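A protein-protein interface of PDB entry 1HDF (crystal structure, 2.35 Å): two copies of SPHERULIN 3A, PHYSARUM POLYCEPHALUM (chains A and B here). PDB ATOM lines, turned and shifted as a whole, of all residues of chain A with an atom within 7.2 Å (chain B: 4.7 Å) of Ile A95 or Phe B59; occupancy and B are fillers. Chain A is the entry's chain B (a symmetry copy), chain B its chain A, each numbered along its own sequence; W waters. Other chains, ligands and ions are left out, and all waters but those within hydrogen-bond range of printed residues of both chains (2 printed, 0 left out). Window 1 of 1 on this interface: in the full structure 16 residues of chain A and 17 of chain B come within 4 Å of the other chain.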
ATOM      1  N   VAL A  15     -10.342  14.783  -8.754  1.00  0.00           N
ATOM      2  CA  VAL A  15     -10.600  15.617  -9.913  1.00  0.00           C
ATOM      3  C   VAL A  15      -9.369  15.556 -10.809  1.00  0.00           C
ATOM      4  O   VAL A  15      -8.238  15.703 -10.347  1.00  0.00           O
ATOM      5  CB  VAL A  15     -10.889  17.070  -9.502  1.00  0.00           C
ATOM      6  CG1 VAL A  15     -10.937  17.967 -10.732  1.00  0.00           C
ATOM      7  CG2 VAL A  15     -12.222  17.131  -8.757  1.00  0.00           C
ATOM      8  N   VAL A  30      -6.368  15.883  -8.326  1.00  0.00           N
ATOM      9  CA  VAL A  30      -6.525  16.705  -7.136  1.00  0.00           C
ATOM     10  C   VAL A  30      -7.618  16.197  -6.204  1.00  0.00           C
ATOM     11  O   VAL A  30      -8.653  15.705  -6.649  1.00  0.00           O
ATOM     12  CB  VAL A  30      -6.876  18.154  -7.522  1.00  0.00           C
ATOM     13  CG1 VAL A  30      -7.040  19.006  -6.266  1.00  0.00           C
ATOM     14  CG2 VAL A  30      -5.801  18.723  -8.420  1.00  0.00           C
ATOM     15  N   THR A  31      -7.366  16.312  -4.905  1.00  0.00           N
ATOM     16  CA  THR A  31      -8.333  15.930  -3.885  1.00  0.00           C
ATOM     17  C   THR A  31      -8.305  17.097  -2.898  1.00  0.00           C
ATOM     18  O   THR A  31      -7.346  17.862  -2.874  1.00  0.00           O
ATOM     19  CB  THR A  31      -7.930  14.626  -3.166  1.00  0.00           C
ATOM     20  OG1 THR A  31      -6.727  14.837  -2.409  1.00  0.00           O
ATOM     21  CG2 THR A  31      -7.696  13.516  -4.185  1.00  0.00           C
ATOM     22  N   GLY A  32      -9.344  17.248  -2.091  1.00  0.00           N
ATOM     23  CA  GLY A  32      -9.363  18.356  -1.153  1.00  0.00           C
ATOM     24  C   GLY A  32      -9.396  19.678  -1.901  1.00  0.00           C
ATOM     25  O   GLY A  32      -9.707  19.709  -3.089  1.00  0.00           O
ATOM     26  N   ASN A  33      -9.057  20.771  -1.224  1.00  0.00           N
ATOM     27  CA  ASN A  33      -9.081  22.079  -1.865  1.00  0.00           C
ATOM     28  C   ASN A  33      -7.694  22.659  -2.174  1.00  0.00           C
ATOM     29  O   ASN A  33      -6.700  22.317  -1.544  1.00  0.00           O
ATOM     30  CB  ASN A  33      -9.856  23.078  -0.997  1.00  0.00           C
ATOM     31  CG  ASN A  33     -11.213  22.549  -0.547  1.00  0.00           C
ATOM     32  OD1 ASN A  33     -11.924  21.879  -1.294  1.00  0.00           O
ATOM     33  ND2 ASN A  33     -11.586  22.876   0.682  1.00  0.00           N
ATOM     34  N   VAL A  34      -7.640  23.536  -3.167  1.00  0.00           N
ATOM     35  CA  VAL A  34      -6.402  24.200  -3.561  1.00  0.00           C
ATOM     36  C   VAL A  34      -6.787  25.659  -3.767  1.00  0.00           C
ATOM     37  O   VAL A  34      -7.450  25.999  -4.749  1.00  0.00           O
ATOM     38  CB  VAL A  34      -5.835  23.627  -4.883  1.00  0.00           C
ATOM     39  CG1 VAL A  34      -4.560  24.380  -5.279  1.00  0.00           C
ATOM     40  CG2 VAL A  34      -5.553  22.139  -4.722  1.00  0.00           C
ATOM     41  N   TYR A  35      -6.388  26.513  -2.829  1.00  0.00           N
ATOM     42  CA  TYR A  35      -6.724  27.929  -2.906  1.00  0.00           C
ATOM     43  C   TYR A  35      -5.795  28.774  -3.784  1.00  0.00           C
ATOM     44  O   TYR A  35      -6.041  29.962  -3.984  1.00  0.00           O
ATOM     45  CB  TYR A  35      -6.818  28.517  -1.492  1.00  0.00           C
ATOM     46  CG  TYR A  35      -5.511  28.581  -0.737  1.00  0.00           C
ATOM     47  CD1 TYR A  35      -4.564  29.570  -1.024  1.00  0.00           C
ATOM     48  CD2 TYR A  35      -5.218  27.658   0.272  1.00  0.00           C
ATOM     49  CE1 TYR A  35      -3.360  29.642  -0.327  1.00  0.00           C
ATOM     50  CE2 TYR A  35      -4.011  27.721   0.979  1.00  0.00           C
ATOM     51  CZ  TYR A  35      -3.090  28.718   0.671  1.00  0.00           C
ATOM     52  OH  TYR A  35      -1.899  28.798   1.351  1.00  0.00           O
ATOM     53  N   PHE A  37      -3.583  27.763  -7.324  1.00  0.00           N
ATOM     54  CA  PHE A  37      -3.013  26.858  -8.319  1.00  0.00           C
ATOM     55  C   PHE A  37      -1.538  27.123  -8.593  1.00  0.00           C
ATOM     56  O   PHE A  37      -0.844  26.282  -9.168  1.00  0.00           O
ATOM     57  CB  PHE A  37      -3.815  26.952  -9.626  1.00  0.00           C
ATOM     58  CG  PHE A  37      -5.004  26.029  -9.679  1.00  0.00           C
ATOM     59  CD1 PHE A  37      -5.667  25.650  -8.508  1.00  0.00           C
ATOM     60  CD2 PHE A  37      -5.463  25.533 -10.900  1.00  0.00           C
ATOM     61  CE1 PHE A  37      -6.763  24.789  -8.555  1.00  0.00           C
ATOM     62  CE2 PHE A  37      -6.559  24.675 -10.956  1.00  0.00           C
ATOM     63  CZ  PHE A  37      -7.211  24.300  -9.785  1.00  0.00           C
ATOM     64  N   THR A  56     -18.996  13.411  -5.950  1.00  0.00           N
ATOM     65  CA  THR A  56     -18.038  14.498  -5.850  1.00  0.00           C
ATOM     66  C   THR A  56     -18.491  15.735  -6.612  1.00  0.00           C
ATOM     67  O   THR A  56     -18.977  15.641  -7.742  1.00  0.00           O
ATOM     68  CB  THR A  56     -16.683  14.062  -6.434  1.00  0.00           C
ATOM     69  OG1 THR A  56     -16.249  12.852  -5.798  1.00  0.00           O
ATOM     70  CG2 THR A  56     -15.642  15.154  -6.238  1.00  0.00           C
ATOM     71  N   LYS A  57     -18.325  16.896  -5.985  1.00  0.00           N
ATOM     72  CA  LYS A  57     -18.670  18.170  -6.608  1.00  0.00           C
ATOM     73  C   LYS A  57     -17.373  18.959  -6.688  1.00  0.00           C
ATOM     74  O   LYS A  57     -16.556  18.908  -5.768  1.00  0.00           O
ATOM     75  CB  LYS A  57     -19.654  18.958  -5.742  1.00  0.00           C
ATOM     76  CG  LYS A  57     -20.918  19.399  -6.445  1.00  0.00           C
ATOM     77  CD  LYS A  57     -21.849  18.220  -6.613  1.00  0.00           C
ATOM     78  CE  LYS A  57     -23.255  18.655  -6.952  1.00  0.00           C
ATOM     79  NZ  LYS A  57     -24.172  17.508  -6.750  1.00  0.00           N
ATOM     80  N   ALA A  58     -17.180  19.689  -7.778  1.00  0.00           N
ATOM     81  CA  ALA A  58     -15.975  20.490  -7.911  1.00  0.00           C
ATOM     82  C   ALA A  58     -16.360  21.927  -8.235  1.00  0.00           C
ATOM     83  O   ALA A  58     -17.345  22.177  -8.933  1.00  0.00           O
ATOM     84  CB  ALA A  58     -15.077  19.918  -8.998  1.00  0.00           C
ATOM     85  N   PHE A  59     -15.595  22.872  -7.699  1.00  0.00           N
ATOM     86  CA  PHE A  59     -15.840  24.281  -7.947  1.00  0.00           C
ATOM     87  C   PHE A  59     -14.527  24.893  -8.403  1.00  0.00           C
ATOM     88  O   PHE A  59     -13.537  24.911  -7.660  1.00  0.00           O
ATOM     89  CB  PHE A  59     -16.366  24.976  -6.689  1.00  0.00           C
ATOM     90  CG  PHE A  59     -17.685  24.430  -6.208  1.00  0.00           C
ATOM     91  CD1 PHE A  59     -17.733  23.273  -5.431  1.00  0.00           C
ATOM     92  CD2 PHE A  59     -18.883  25.040  -6.574  1.00  0.00           C
ATOM     93  CE1 PHE A  59     -18.962  22.725  -5.025  1.00  0.00           C
ATOM     94  CE2 PHE A  59     -20.118  24.502  -6.175  1.00  0.00           C
ATOM     95  CZ  PHE A  59     -20.155  23.341  -5.400  1.00  0.00           C
ATOM     96  N   ILE A  60     -14.524  25.376  -9.643  1.00  0.00           N
ATOM     97  CA  ILE A  60     -13.335  25.960 -10.231  1.00  0.00           C
ATOM     98  C   ILE A  60     -13.474  27.457 -10.357  1.00  0.00           C
ATOM     99  O   ILE A  60     -14.452  27.961 -10.898  1.00  0.00           O
ATOM    100  CB  ILE A  60     -13.054  25.335 -11.597  1.00  0.00           C
ATOM    101  CG1 ILE A  60     -14.306  25.411 -12.476  1.00  0.00           C
ATOM    102  CG2 ILE A  60     -12.637  23.883 -11.407  1.00  0.00           C
ATOM    103  CD1 ILE A  60     -14.133  24.824 -13.862  1.00  0.00           C
ATOM    104  N   PHE A  61     -12.477  28.165  -9.848  1.00  0.00           N
ATOM    105  CA  PHE A  61     -12.506  29.611  -9.867  1.00  0.00           C
ATOM    106  C   PHE A  61     -11.465  30.198 -10.788  1.00  0.00           C
ATOM    107  O   PHE A  61     -10.380  29.632 -10.968  1.00  0.00           O
ATOM    108  CB  PHE A  61     -12.296  30.147  -8.448  1.00  0.00           C
ATOM    109  CG  PHE A  61     -13.263  29.599  -7.460  1.00  0.00           C
ATOM    110  CD1 PHE A  61     -13.200  28.262  -7.080  1.00  0.00           C
ATOM    111  CD2 PHE A  61     -14.272  30.405  -6.939  1.00  0.00           C
ATOM    112  CE1 PHE A  61     -14.128  27.736  -6.199  1.00  0.00           C
ATOM    113  CE2 PHE A  61     -15.206  29.888  -6.056  1.00  0.00           C
ATOM    114  CZ  PHE A  61     -15.136  28.553  -5.685  1.00  0.00           C
ATOM    115  N   ARG A  65      -7.776  31.855  -4.260  1.00  0.00           N
ATOM    116  CA  ARG A  65      -8.577  32.051  -3.057  1.00  0.00           C
ATOM    117  C   ARG A  65     -10.089  32.061  -3.296  1.00  0.00           C
ATOM    118  O   ARG A  65     -10.848  32.758  -2.613  1.00  0.00           O
ATOM    119  CB  ARG A  65      -8.106  33.327  -2.356  1.00  0.00           C
ATOM    120  CG  ARG A  65      -6.638  33.206  -1.936  1.00  0.00           C
ATOM    121  CD  ARG A  65      -6.045  34.473  -1.342  1.00  0.00           C
ATOM    122  NE  ARG A  65      -4.724  34.214  -0.774  1.00  0.00           N
ATOM    123  CZ  ARG A  65      -3.648  33.877  -1.482  1.00  0.00           C
ATOM    124  NH1 ARG A  65      -3.729  33.760  -2.801  1.00  0.00           N
ATOM    125  NH2 ARG A  65      -2.492  33.640  -0.870  1.00  0.00           N
ATOM    126  N   PHE A  66     -10.510  31.273  -4.280  1.00  0.00           N
ATOM    127  CA  PHE A  66     -11.921  31.127  -4.631  1.00  0.00           C
ATOM    128  C   PHE A  66     -12.623  32.436  -4.988  1.00  0.00           C
ATOM    129  O   PHE A  66     -13.787  32.650  -4.625  1.00  0.00           O
ATOM    130  CB  PHE A  66     -12.656  30.427  -3.479  1.00  0.00           C
ATOM    131  CG  PHE A  66     -11.805  29.422  -2.760  1.00  0.00           C
ATOM    132  CD1 PHE A  66     -11.347  28.285  -3.423  1.00  0.00           C
ATOM    133  CD2 PHE A  66     -11.400  29.644  -1.445  1.00  0.00           C
ATOM    134  CE1 PHE A  66     -10.499  27.391  -2.792  1.00  0.00           C
ATOM    135  CE2 PHE A  66     -10.553  28.757  -0.803  1.00  0.00           C
ATOM    136  CZ  PHE A  66     -10.098  27.628  -1.476  1.00  0.00           C
ATOM    137  N   ASN A  67     -11.916  33.301  -5.708  1.00  0.00           N
ATOM    138  CA  ASN A  67     -12.472  34.581  -6.141  1.00  0.00           C
ATOM    139  C   ASN A  67     -12.746  34.539  -7.641  1.00  0.00           C
ATOM    140  O   ASN A  67     -12.385  33.575  -8.316  1.00  0.00           O
ATOM    141  CB  ASN A  67     -11.503  35.724  -5.836  1.00  0.00           C
ATOM    142  CG  ASN A  67     -11.321  35.949  -4.351  1.00  0.00           C
ATOM    143  OD1 ASN A  67     -12.298  36.114  -3.617  1.00  0.00           O
ATOM    144  ND2 ASN A  67     -10.068  35.967  -3.899  1.00  0.00           N
ATOM    145  N   PHE A  70     -16.781  31.564 -11.438  1.00  0.00           N
ATOM    146  CA  PHE A  70     -16.620  30.150 -11.130  1.00  0.00           C
ATOM    147  C   PHE A  70     -17.866  29.347 -11.489  1.00  0.00           C
ATOM    148  O   PHE A  70     -18.938  29.909 -11.686  1.00  0.00           O
ATOM    149  CB  PHE A  70     -16.323  29.988  -9.637  1.00  0.00           C
ATOM    150  CG  PHE A  70     -17.499  30.299  -8.739  1.00  0.00           C
ATOM    151  CD1 PHE A  70     -17.790  31.607  -8.383  1.00  0.00           C
ATOM    152  CD2 PHE A  70     -18.314  29.276  -8.252  1.00  0.00           C
ATOM    153  CE1 PHE A  70     -18.868  31.903  -7.557  1.00  0.00           C
ATOM    154  CE2 PHE A  70     -19.398  29.559  -7.421  1.00  0.00           C
ATOM    155  CZ  PHE A  70     -19.678  30.878  -7.072  1.00  0.00           C
ATOM    156  N   SER A  93      -7.985  28.420  -8.619  1.00  0.00           N
ATOM    157  CA  SER A  93      -8.307  27.841  -7.318  1.00  0.00           C
ATOM    158  C   SER A  93      -9.458  26.857  -7.504  1.00  0.00           C
ATOM    159  O   SER A  93     -10.202  26.942  -8.485  1.00  0.00           O
ATOM    160  CB  SER A  93      -8.641  28.923  -6.269  1.00  0.00           C
ATOM    161  OG  SER A  93      -9.743  29.742  -6.622  1.00  0.00           O
ATOM    162  N   MET A  94      -9.593  25.905  -6.585  1.00  0.00           N
ATOM    163  CA  MET A  94     -10.633  24.906  -6.720  1.00  0.00           C
ATOM    164  C   MET A  94     -11.017  24.254  -5.407  1.00  0.00           C
ATOM    165  O   MET A  94     -10.191  24.103  -4.510  1.00  0.00           O
ATOM    166  CB  MET A  94     -10.182  23.822  -7.718  1.00  0.00           C
ATOM    167  CG  MET A  94     -11.097  22.602  -7.805  1.00  0.00           C
ATOM    168  SD  MET A  94     -10.690  21.409  -9.304  1.00  0.00           S
ATOM    169  CE  MET A  94      -9.230  20.431  -8.523  1.00  0.00           C
ATOM    170  N   ILE A  95     -12.287  23.878  -5.315  1.00  0.00           N
ATOM    171  CA  ILE A  95     -12.832  23.199  -4.152  1.00  0.00           C
ATOM    172  C   ILE A  95     -13.322  21.831  -4.601  1.00  0.00           C
ATOM    173  O   ILE A  95     -14.011  21.705  -5.611  1.00  0.00           O
ATOM    174  CB  ILE A  95     -14.024  23.976  -3.524  1.00  0.00           C
ATOM    175  CG1 ILE A  95     -13.507  25.208  -2.778  1.00  0.00           C
ATOM    176  CG2 ILE A  95     -14.797  23.070  -2.567  1.00  0.00           C
ATOM    177  CD1 ILE A  95     -14.586  26.027  -2.100  1.00  0.00           C
ATOM    178  N   VAL A  96     -12.942  20.805  -3.855  1.00  0.00           N
ATOM    179  CA  VAL A  96     -13.353  19.446  -4.169  1.00  0.00           C
ATOM    180  C   VAL A  96     -14.114  18.925  -2.963  1.00  0.00           C
ATOM    181  O   VAL A  96     -13.520  18.646  -1.927  1.00  0.00           O
ATOM    182  CB  VAL A  96     -12.126  18.539  -4.436  1.00  0.00           C
ATOM    183  CG1 VAL A  96     -12.583  17.129  -4.786  1.00  0.00           C
ATOM    184  CG2 VAL A  96     -11.285  19.131  -5.569  1.00  0.00           C
ATOM    185  N   ALA A  97     -15.430  18.810  -3.088  1.00  0.00           N
ATOM    186  CA  ALA A  97     -16.241  18.337  -1.981  1.00  0.00           C
ATOM    187  C   ALA A  97     -16.938  17.039  -2.326  1.00  0.00           C
ATOM    188  O   ALA A  97     -17.387  16.843  -3.455  1.00  0.00           O
ATOM    189  CB  ALA A  97     -17.265  19.395  -1.596  1.00  0.00           C
ATOM    190  N   LYS B  57     -14.413  31.311   2.910  1.00  0.00           N
ATOM    191  CA  LYS B  57     -15.450  31.470   1.903  1.00  0.00           C
ATOM    192  C   LYS B  57     -16.529  30.476   2.294  1.00  0.00           C
ATOM    193  O   LYS B  57     -16.231  29.409   2.834  1.00  0.00           O
ATOM    194  CB  LYS B  57     -14.934  31.125   0.508  1.00  0.00           C
ATOM    195  CG  LYS B  57     -15.053  32.250  -0.505  1.00  0.00           C
ATOM    196  CD  LYS B  57     -14.056  33.358  -0.216  1.00  0.00           C
ATOM    197  CE  LYS B  57     -13.868  34.255  -1.424  1.00  0.00           C
ATOM    198  NZ  LYS B  57     -12.749  35.212  -1.207  1.00  0.00           N
ATOM    199  N   ALA B  58     -17.780  30.828   2.036  1.00  0.00           N
ATOM    200  CA  ALA B  58     -18.877  29.935   2.349  1.00  0.00           C
ATOM    201  C   ALA B  58     -19.799  29.835   1.144  1.00  0.00           C
ATOM    202  O   ALA B  58     -20.139  30.842   0.523  1.00  0.00           O
ATOM    203  CB  ALA B  58     -19.639  30.448   3.549  1.00  0.00           C
ATOM    204  N   PHE B  59     -20.184  28.613   0.804  1.00  0.00           N
ATOM    205  CA  PHE B  59     -21.085  28.381  -0.313  1.00  0.00           C
ATOM    206  C   PHE B  59     -22.332  27.668   0.214  1.00  0.00           C
ATOM    207  O   PHE B  59     -22.270  26.522   0.669  1.00  0.00           O
ATOM    208  CB  PHE B  59     -20.387  27.541  -1.387  1.00  0.00           C
ATOM    209  CG  PHE B  59     -19.150  28.192  -1.960  1.00  0.00           C
ATOM    210  CD1 PHE B  59     -17.939  28.143  -1.277  1.00  0.00           C
ATOM    211  CD2 PHE B  59     -19.206  28.878  -3.167  1.00  0.00           C
ATOM    212  CE1 PHE B  59     -16.796  28.772  -1.790  1.00  0.00           C
ATOM    213  CE2 PHE B  59     -18.073  29.509  -3.687  1.00  0.00           C
ATOM    214  CZ  PHE B  59     -16.865  29.454  -2.993  1.00  0.00           C
ATOM    215  N   ILE B  60     -23.461  28.361   0.169  1.00  0.00           N
ATOM    216  CA  ILE B  60     -24.721  27.808   0.652  1.00  0.00           C
ATOM    217  C   ILE B  60     -25.592  27.349  -0.519  1.00  0.00           C
ATOM    218  O   ILE B  60     -25.774  28.079  -1.488  1.00  0.00           O
ATOM    219  CB  ILE B  60     -25.467  28.859   1.496  1.00  0.00           C
ATOM    220  CG1 ILE B  60     -25.617  30.156   0.692  1.00  0.00           C
ATOM    221  CG2 ILE B  60     -24.705  29.121   2.787  1.00  0.00           C
ATOM    222  CD1 ILE B  60     -26.397  31.234   1.414  1.00  0.00           C
ATOM    223  N   PHE B  61     -26.127  26.135  -0.416  1.00  0.00           N
ATOM    224  CA  PHE B  61     -26.953  25.550  -1.472  1.00  0.00           C
ATOM    225  C   PHE B  61     -28.393  25.324  -1.053  1.00  0.00           C
ATOM    226  O   PHE B  61     -28.668  24.975   0.099  1.00  0.00           O
ATOM    227  CB  PHE B  61     -26.345  24.223  -1.924  1.00  0.00           C
ATOM    228  CG  PHE B  61     -24.944  24.358  -2.408  1.00  0.00           C
ATOM    229  CD1 PHE B  61     -23.909  24.608  -1.506  1.00  0.00           C
ATOM    230  CD2 PHE B  61     -24.665  24.339  -3.771  1.00  0.00           C
ATOM    231  CE1 PHE B  61     -22.623  24.843  -1.955  1.00  0.00           C
ATOM    232  CE2 PHE B  61     -23.380  24.575  -4.231  1.00  0.00           C
ATOM    233  CZ  PHE B  61     -22.357  24.829  -3.326  1.00  0.00           C
ATOM    234  N   ILE B  71     -25.020  30.546  -3.596  1.00  0.00           N
ATOM    235  CA  ILE B  71     -24.263  31.790  -3.673  1.00  0.00           C
ATOM    236  C   ILE B  71     -22.995  31.697  -2.834  1.00  0.00           C
ATOM    237  O   ILE B  71     -22.918  30.922  -1.874  1.00  0.00           O
ATOM    238  CB  ILE B  71     -25.064  33.014  -3.156  1.00  0.00           C
ATOM    239  CG1 ILE B  71     -25.387  32.841  -1.672  1.00  0.00           C
ATOM    240  CG2 ILE B  71     -26.333  33.214  -3.999  1.00  0.00           C
ATOM    241  CD1 ILE B  71     -25.881  34.107  -1.000  1.00  0.00           C
ATOM    242  N   ARG B  72     -22.003  32.496  -3.204  1.00  0.00           N
ATOM    243  CA  ARG B  72     -20.745  32.535  -2.482  1.00  0.00           C
ATOM    244  C   ARG B  72     -20.765  33.635  -1.423  1.00  0.00           C
ATOM    245  O   ARG B  72     -21.194  34.762  -1.693  1.00  0.00           O
ATOM    246  CB  ARG B  72     -19.595  32.786  -3.458  1.00  0.00           C
ATOM    247  CG  ARG B  72     -18.282  33.169  -2.792  1.00  0.00           C
ATOM    248  CD  ARG B  72     -17.197  33.388  -3.837  1.00  0.00           C
ATOM    249  NE  ARG B  72     -17.619  34.357  -4.841  1.00  0.00           N
ATOM    250  CZ  ARG B  72     -17.048  34.494  -6.030  1.00  0.00           C
ATOM    251  NH1 ARG B  72     -16.021  33.721  -6.364  1.00  0.00           N
ATOM    252  NH2 ARG B  72     -17.513  35.390  -6.892  1.00  0.00           N
ATOM    253  N   SER B  93     -27.316  22.462   2.336  1.00  0.00           N
ATOM    254  CA  SER B  93     -25.931  21.993   2.294  1.00  0.00           C
ATOM    255  C   SER B  93     -25.024  23.220   2.233  1.00  0.00           C
ATOM    256  O   SER B  93     -25.467  24.314   1.888  1.00  0.00           O
ATOM    257  CB  SER B  93     -25.676  21.059   1.093  1.00  0.00           C
ATOM    258  OG  SER B  93     -25.855  21.701  -0.153  1.00  0.00           O
ATOM    259  N   MET B  94     -23.756  23.044   2.575  1.00  0.00           N
ATOM    260  CA  MET B  94     -22.848  24.167   2.571  1.00  0.00           C
ATOM    261  C   MET B  94     -21.396  23.718   2.565  1.00  0.00           C
ATOM    262  O   MET B  94     -21.063  22.676   3.120  1.00  0.00           O
ATOM    263  CB  MET B  94     -23.133  25.044   3.801  1.00  0.00           C
ATOM    264  CG  MET B  94     -22.191  26.221   3.992  1.00  0.00           C
ATOM    265  SD  MET B  94     -22.744  27.431   5.415  1.00  0.00           S
ATOM    266  CE  MET B  94     -22.097  26.425   6.922  1.00  0.00           C
ATOM    267  N   ILE B  95     -20.552  24.509   1.908  1.00  0.00           N
ATOM    268  CA  ILE B  95     -19.115  24.257   1.825  1.00  0.00           C
ATOM    269  C   ILE B  95     -18.389  25.419   2.499  1.00  0.00           C
ATOM    270  O   ILE B  95     -18.656  26.590   2.202  1.00  0.00           O
ATOM    271  CB  ILE B  95     -18.625  24.171   0.351  1.00  0.00           C
ATOM    272  CG1 ILE B  95     -19.100  22.865  -0.288  1.00  0.00           C
ATOM    273  CG2 ILE B  95     -17.110  24.239   0.303  1.00  0.00           C
ATOM    274  CD1 ILE B  95     -18.758  22.731  -1.755  1.00  0.00           C
ATOM    275  N   ALA B  97     -14.682  26.863   3.031  1.00  0.00           N
ATOM    276  CA  ALA B  97     -13.301  26.744   2.579  1.00  0.00           C
ATOM    277  C   ALA B  97     -12.446  27.916   3.036  1.00  0.00           C
ATOM    278  O   ALA B  97     -12.888  29.066   3.022  1.00  0.00           O
ATOM    279  CB  ALA B  97     -13.265  26.626   1.060  1.00  0.00           C
HETATM  280  O   HOH W   1     -14.888  36.150  -4.167  1.00  0.00           O
HETATM  281  O   HOH W   2     -10.088  36.789  -0.916  1.00  0.00           O
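The side-chain amino group (NZ) of Lys B57 lies within hydrogen-bond range of the side-chain amide oxygen (OD1) of Asn A67 (2.6 Å). O of Phe A66 sits at hydrogen-bond distance from NH1 of Arg B72 (3.0 Å). The side-chain amino group (NZ) of Lys B57 lies within hydrogen-bond range of the backbone carbonyl oxygen (O) of Arg A65, at 3.4 Å.
O of Ser A93 sits at hydrogen-bond distance from N of Phe A61. N of Phe B59 sits at hydrogen-bond distance from O of Ile B95, at 2.9 Å. N of Lys B57 sits at hydrogen-bond distance from O of Ala B97, at 2.7 Å. The backbone carbonyl oxygen (O) of Tyr A35 is in hydrogen-bond range of the backbone NH (N) of Arg A65, 2.6 Å away. The backbone carbonyl oxygen (O) of Phe A59 sits at hydrogen-bond distance from the backbone NH (N) of Ile A95, at 2.9 Å. O of Ser B93 lies within hydrogen-bond range of N of Phe B61 (3.0 Å).
Among the printed residues, pairs that only touch across the chains: Phe A59 with Phe B61, Phe A59 with Ile B95, Phe A61 with Phe B59, Phe A61 with Arg B72, Phe A66 with Lys B57, Phe A66 with Ala B97, Asn A67 with Arg B72, Phe A70 with Phe B59, Phe A70 with Arg B72, Ile A95 with Phe B59, Ile A95 with Ile B95, Ile A95 with Ala B97 and Ala A97 with Ile B95.
Ile A95 touches just these residues of chain B: Phe B59 (3.5 Å), Ile B95 (3.9 Å) and Ala B97 (3.5 Å). Printed residues of chain A within 4 Å of Phe B59: Phe A61, Phe A70 and Ile A95. Of the printed residues of chain B, Phe A59 touches Phe B61 (3.4 Å) and Ile B95 (3.3 Å). Of the printed residues of chain A, Lys B57 touches Arg A65 (3.4 Å), Phe A66 (3.6 Å) and Asn A67 (2.6 Å). Printed residues of chain A within 4 Å of Ile B95: Phe A59 (3.3 Å), Ile A95 (3.9 Å) and Ala A97 (3.7 Å). Of the printed residues of chain A, Ala B97 touches Phe A66 (3.9 Å) and Ile A95 (3.5 Å). Printed residues of chain B within 4 Å of Ala A97: Ile B95. The nearest printed residue of chain B that does not touch Ile A95 is Lys B57 (5.7 Å).
Of the 23 printed residues of chain A, 8 touch a printed residue of chain B. Hydrophobic or aromatic side chains of chain A that line the printed part of chain B: Phe A59, Phe A61, Phe A66, Phe A70, Ile A95 and Ala A97. Along chain B the printed residues that touch a printed residue of chain A span positions 57 to 97.
Phe A59 touches Phe B61, and with the chains exchanged Phe A61 touches Phe B59. Phe A59 touches Ile B95, and with the chains exchanged Ile A95 touches Phe B59. Ile A95 touches its own counterpart, Ile B95. Ile A95 touches Ala B97, and with the chains exchanged Ala A97 touches Ile B95. 9 positions are printed for both chains. Of the 16 pairs that touch across the chains among the printed residues, 7 have their exchanged pair printed and touching as well.
Water W1 lies within hydrogen-bond range of OD1 of Asn A67 (2.6 Å) and NE of Arg B72 (3.3 Å). Water W2 lies within hydrogen-bond range of ND2 of Asn A67 (3.1 Å) and NZ of Lys B57 (3.1 Å).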
